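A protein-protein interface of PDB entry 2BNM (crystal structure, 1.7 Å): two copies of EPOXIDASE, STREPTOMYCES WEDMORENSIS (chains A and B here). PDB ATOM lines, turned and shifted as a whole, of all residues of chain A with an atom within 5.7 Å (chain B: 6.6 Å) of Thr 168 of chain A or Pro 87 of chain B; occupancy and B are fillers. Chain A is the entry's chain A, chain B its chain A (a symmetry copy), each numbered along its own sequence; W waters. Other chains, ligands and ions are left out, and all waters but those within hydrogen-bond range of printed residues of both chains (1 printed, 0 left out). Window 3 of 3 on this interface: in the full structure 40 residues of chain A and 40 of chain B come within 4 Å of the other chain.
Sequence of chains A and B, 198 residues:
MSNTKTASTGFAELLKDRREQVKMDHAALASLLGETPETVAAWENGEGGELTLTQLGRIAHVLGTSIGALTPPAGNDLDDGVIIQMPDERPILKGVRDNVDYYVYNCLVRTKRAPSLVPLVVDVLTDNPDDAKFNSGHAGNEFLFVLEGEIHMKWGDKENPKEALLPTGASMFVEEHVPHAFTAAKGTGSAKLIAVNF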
ATOM      1  N   VAL A 146       4.820 -13.688  -2.196  1.00  0.00           N
ATOM      2  CA  VAL A 146       4.886 -15.122  -2.586  1.00  0.00           C
ATOM      3  C   VAL A 146       3.804 -15.863  -1.801  1.00  0.00           C
ATOM      4  O   VAL A 146       3.850 -15.967  -0.574  1.00  0.00           O
ATOM      5  CB  VAL A 146       6.278 -15.749  -2.370  1.00  0.00           C
ATOM      6  CG1 VAL A 146       6.273 -17.257  -2.828  1.00  0.00           C
ATOM      7  CG2 VAL A 146       7.352 -15.023  -3.139  1.00  0.00           C
ATOM      8  N   LEU A 147       2.769 -16.284  -2.525  1.00  0.00           N
ATOM      9  CA  LEU A 147       1.593 -16.892  -1.924  1.00  0.00           C
ATOM     10  C   LEU A 147       1.806 -18.366  -1.645  1.00  0.00           C
ATOM     11  O   LEU A 147       1.364 -18.867  -0.616  1.00  0.00           O
ATOM     12  CB  LEU A 147       0.457 -16.844  -2.935  1.00  0.00           C
ATOM     13  CG  LEU A 147      -0.487 -15.687  -2.891  1.00  0.00           C
ATOM     14  CD1 LEU A 147      -1.655 -16.022  -3.818  1.00  0.00           C
ATOM     15  CD2 LEU A 147      -0.981 -15.505  -1.469  1.00  0.00           C
ATOM     16  N   GLU A 148       2.491 -19.041  -2.566  1.00  0.00           N
ATOM     17  CA  GLU A 148       2.701 -20.481  -2.476  1.00  0.00           C
ATOM     18  C   GLU A 148       4.027 -20.893  -3.084  1.00  0.00           C
ATOM     19  O   GLU A 148       4.461 -20.360  -4.119  1.00  0.00           O
ATOM     20  CB  GLU A 148       1.569 -21.234  -3.194  1.00  0.00           C
ATOM     21  CG  GLU A 148       0.295 -21.356  -2.378  1.00  0.00           C
ATOM     22  CD  GLU A 148      -0.839 -22.073  -3.101  1.00  0.00           C
ATOM     23  OE1 GLU A 148      -0.584 -22.781  -4.098  1.00  0.00           O
ATOM     24  OE2 GLU A 148      -2.001 -21.924  -2.658  1.00  0.00           O
ATOM     25  N   GLY A 149       4.685 -21.866  -2.471  1.00  0.00           N
ATOM     26  CA  GLY A 149       5.904 -22.349  -3.057  1.00  0.00           C
ATOM     27  C   GLY A 149       7.067 -21.402  -2.841  1.00  0.00           C
ATOM     28  O   GLY A 149       7.059 -20.594  -1.911  1.00  0.00           O
ATOM     29  N   GLU A 150       8.035 -21.510  -3.734  1.00  0.00           N
ATOM     30  CA  GLU A 150       9.305 -20.795  -3.644  1.00  0.00           C
ATOM     31  C   GLU A 150       9.631 -20.221  -5.004  1.00  0.00           C
ATOM     32  O   GLU A 150       9.606 -20.928  -6.013  1.00  0.00           O
ATOM     33  CB  GLU A 150      10.415 -21.759  -3.185  1.00  0.00           C
ATOM     34  CG  GLU A 150      11.768 -21.093  -3.008  1.00  0.00           C
ATOM     35  CD  GLU A 150      12.864 -22.087  -2.671  1.00  0.00           C
ATOM     36  OE1 GLU A 150      12.581 -23.317  -2.631  1.00  0.00           O
ATOM     37  OE2 GLU A 150      13.998 -21.624  -2.447  1.00  0.00           O
ATOM     38  N   LEU A 166      12.979 -16.693  -3.081  1.00  0.00           N
ATOM     39  CA  LEU A 166      11.974 -16.070  -2.234  1.00  0.00           C
ATOM     40  C   LEU A 166      10.991 -17.122  -1.753  1.00  0.00           C
ATOM     41  O   LEU A 166      10.176 -17.602  -2.539  1.00  0.00           O
ATOM     42  CB  LEU A 166      11.261 -14.978  -3.046  1.00  0.00           C
ATOM     43  CG  LEU A 166      12.211 -13.907  -3.635  1.00  0.00           C
ATOM     44  CD1 LEU A 166      11.512 -13.140  -4.727  1.00  0.00           C
ATOM     45  CD2 LEU A 166      12.664 -12.965  -2.523  1.00  0.00           C
ATOM     46  N   PRO A 167      11.058 -17.474  -0.474  1.00  0.00           N
ATOM     47  CA  PRO A 167      10.147 -18.463   0.099  1.00  0.00           C
ATOM     48  C   PRO A 167       8.762 -17.883   0.242  1.00  0.00           C
ATOM     49  O   PRO A 167       8.572 -16.654   0.122  1.00  0.00           O
ATOM     50  CB  PRO A 167      10.733 -18.712   1.489  1.00  0.00           C
ATOM     51  CG  PRO A 167      11.425 -17.457   1.825  1.00  0.00           C
ATOM     52  CD  PRO A 167      12.036 -16.983   0.522  1.00  0.00           C
ATOM     53  N   THR A 168       7.788 -18.746   0.483  1.00  0.00           N
ATOM     54  CA  THR A 168       6.424 -18.306   0.765  1.00  0.00           C
ATOM     55  C   THR A 168       6.406 -17.192   1.813  1.00  0.00           C
ATOM     56  O   THR A 168       7.032 -17.304   2.884  1.00  0.00           O
ATOM     57  CB  THR A 168       5.581 -19.494   1.242  1.00  0.00           C
ATOM     58  OG1 THR A 168       5.459 -20.424   0.162  1.00  0.00           O
ATOM     59  CG2 THR A 168       4.144 -19.069   1.486  1.00  0.00           C
ATOM     60  N   GLY A 169       5.692 -16.112   1.501  1.00  0.00           N
ATOM     61  CA  GLY A 169       5.562 -15.042   2.477  1.00  0.00           C
ATOM     62  C   GLY A 169       6.532 -13.894   2.202  1.00  0.00           C
ATOM     63  O   GLY A 169       6.386 -12.840   2.807  1.00  0.00           O
ATOM     64  N   ALA A 170       7.528 -14.120   1.340  1.00  0.00           N
ATOM     65  CA  ALA A 170       8.465 -13.035   0.982  1.00  0.00           C
ATOM     66  C   ALA A 170       7.686 -11.983   0.203  1.00  0.00           C
ATOM     67  O   ALA A 170       6.663 -12.290  -0.428  1.00  0.00           O
ATOM     68  CB  ALA A 170       9.605 -13.554   0.145  1.00  0.00           C
ATOM     69  N   GLN B  85      12.026  -8.468   0.843  1.00  0.00           N
ATOM     70  CA  GLN B  85      11.939  -8.735   2.263  1.00  0.00           C
ATOM     71  C   GLN B  85      11.624 -10.221   2.472  1.00  0.00           C
ATOM     72  O   GLN B  85      10.645 -10.761   1.938  1.00  0.00           O
ATOM     73  CB  GLN B  85      10.861  -7.894   2.889  1.00  0.00           C
ATOM     74  CG  GLN B  85      10.650  -8.143   4.356  1.00  0.00           C
ATOM     75  CD  GLN B  85       9.252  -7.763   4.765  1.00  0.00           C
ATOM     76  OE1 GLN B  85       8.287  -8.282   4.202  1.00  0.00           O
ATOM     77  NE2 GLN B  85       9.133  -6.822   5.684  1.00  0.00           N
ATOM     78  N   MET B  86      12.440 -10.881   3.284  1.00  0.00           N
ATOM     79  CA  MET B  86      12.173 -12.274   3.635  1.00  0.00           C
ATOM     80  C   MET B  86      11.157 -12.319   4.763  1.00  0.00           C
ATOM     81  O   MET B  86      11.083 -11.386   5.558  1.00  0.00           O
ATOM     82  CB  MET B  86      13.487 -12.946   4.058  1.00  0.00           C
ATOM     83  CG  MET B  86      14.553 -12.909   2.956  1.00  0.00           C
ATOM     84  SD  MET B  86      14.134 -13.964   1.546  1.00  0.00           S
ATOM     85  CE  MET B  86      14.688 -15.531   2.196  1.00  0.00           C
ATOM     86  N   PRO B  87      10.365 -13.391   4.869  1.00  0.00           N
ATOM     87  CA  PRO B  87       9.299 -13.424   5.868  1.00  0.00           C
ATOM     88  C   PRO B  87       9.772 -13.312   7.325  1.00  0.00           C
ATOM     89  O   PRO B  87       9.064 -12.747   8.147  1.00  0.00           O
ATOM     90  CB  PRO B  87       8.557 -14.749   5.581  1.00  0.00           C
ATOM     91  CG  PRO B  87       9.426 -15.532   4.714  1.00  0.00           C
ATOM     92  CD  PRO B  87      10.393 -14.608   4.033  1.00  0.00           C
ATOM     93  N   ASP B  88      10.980 -13.785   7.622  1.00  0.00           N
ATOM     94  CA  ASP B  88      11.527 -13.656   8.978  1.00  0.00           C
ATOM     95  C   ASP B  88      11.837 -12.192   9.365  1.00  0.00           C
ATOM     96  O   ASP B  88      11.982 -11.881  10.557  1.00  0.00           O
ATOM     97  CB  ASP B  88      12.835 -14.458   9.084  1.00  0.00           C
ATOM     98  CG  ASP B  88      12.631 -15.963   8.970  1.00  0.00           C
ATOM     99  OD1 ASP B  88      11.638 -16.410   8.354  1.00  0.00           O
ATOM    100  OD2 ASP B  88      13.440 -16.782   9.461  1.00  0.00           O
ATOM    101  N   GLU B  89      11.956 -11.319   8.356  1.00  0.00           N
ATOM    102  CA  GLU B  89      12.362  -9.903   8.523  1.00  0.00           C
ATOM    103  C   GLU B  89      11.233  -8.944   8.884  1.00  0.00           C
ATOM    104  O   GLU B  89      11.495  -7.775   9.182  1.00  0.00           O
ATOM    105  CB  GLU B  89      12.905  -9.321   7.207  1.00  0.00           C
ATOM    106  CG  GLU B  89      14.113  -9.924   6.513  1.00  0.00           C
ATOM    107  CD  GLU B  89      14.482  -9.098   5.279  1.00  0.00           C
ATOM    108  OE1 GLU B  89      14.410  -7.848   5.353  1.00  0.00           O
ATOM    109  OE2 GLU B  89      14.852  -9.666   4.234  1.00  0.00           O
ATOM    110  N   ARG B  90       9.978  -9.370   8.782  1.00  0.00           N
ATOM    111  CA  ARG B  90       8.882  -8.413   8.904  1.00  0.00           C
ATOM    112  C   ARG B  90       8.874  -7.788  10.272  1.00  0.00           C
ATOM    113  O   ARG B  90       8.972  -8.516  11.280  1.00  0.00           O
ATOM    114  CB  ARG B  90       7.531  -9.089   8.726  1.00  0.00           C
ATOM    115  CG  ARG B  90       7.337  -9.745   7.413  1.00  0.00           C
ATOM    116  CD  ARG B  90       6.252 -10.733   7.491  1.00  0.00           C
ATOM    117  NE  ARG B  90       5.996 -11.422   6.241  1.00  0.00           N
ATOM    118  CZ  ARG B  90       4.943 -12.199   6.088  1.00  0.00           C
ATOM    119  NH1 ARG B  90       4.105 -12.349   7.113  1.00  0.00           N
ATOM    120  NH2 ARG B  90       4.729 -12.817   4.941  1.00  0.00           N
HETATM  121  O   HOH W   1       7.769 -10.740   3.958  1.00  0.00           O
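Printed residues of chain B that touch a printed residue of chain A: Gln 85, Met 86, Pro 87 and Arg 90. Hydrophobic or aromatic side chains of chain B that line the printed part of chain A: Met 86 and Pro 87. Of the 10 printed residues of chain A, 4 touch a printed residue of chain B. Hydrophobic or aromatic side chains of chain A within 4 Å of the printed part of chain B: Pro 167 and Ala 170.
Water W1 lies within hydrogen-bond range of the side-chain amide oxygen (OE1) of Gln 85 of chain B, the backbone carbonyl oxygen (O) of Gly 169 of chain A and the guanidinium group (NE) of Arg 90 of chain B.
No position is printed for both chains. Of the 6 pairs that touch across the chains among the printed residues, none has its exchanged pair printed and touching as well.
Met 86 of chain B touches Pro 167 of chain A. Pro 87 of chain B touches Pro 167 of chain A. Pro 87 of chain B touches Thr 168 of chain A. Gln 85 of chain B touches Ala 170 of chain A. Ala 170 of chain A touches Pro 87 of chain B (CA to CD, 3.9 Å).
The side-chain hydroxyl (OG1) of Thr 168 of chain A lies within hydrogen-bond range of the backbone carbonyl oxygen (O) of Gly 149 of chain A (2.6 Å). OE2 of Glu 89 of chain B sits at hydrogen-bond distance from N of Met 86 of chain B (2.9 Å). O of Val 146 of chain A is in hydrogen-bond range of N of Gly 169 of chain A (2.8 Å). O of Ala 170 of chain A is in hydrogen-bond range of N of Val 146 of chain A (2.9 Å).
Gly 149 of chain A touches none of the printed residues of chain B. Of the printed residues of chain B, Thr 168 of chain A touches Pro 87 (3.5 Å). Printed residues of chain B within 4 Å of Gly 169 of chain A: Arg 90 (2.7 Å). Of the printed residues of chain A, Gln 85 of chain B touches Ala 170 (3.3 Å). Printed residues of chain A within 4 Å of Met 86 of chain B: Pro 167. Of the printed residues of chain A, Pro 87 of chain B touches Pro 167 (3.7 Å), Thr 168 (3.5 Å) and Ala 170 (3.9 Å).
The backbone carbonyl oxygen (O) of Gly 169 of chain A sits at hydrogen-bond distance from the guanidinium group (NH2) of Arg 90 of chain B (2.7 Å).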
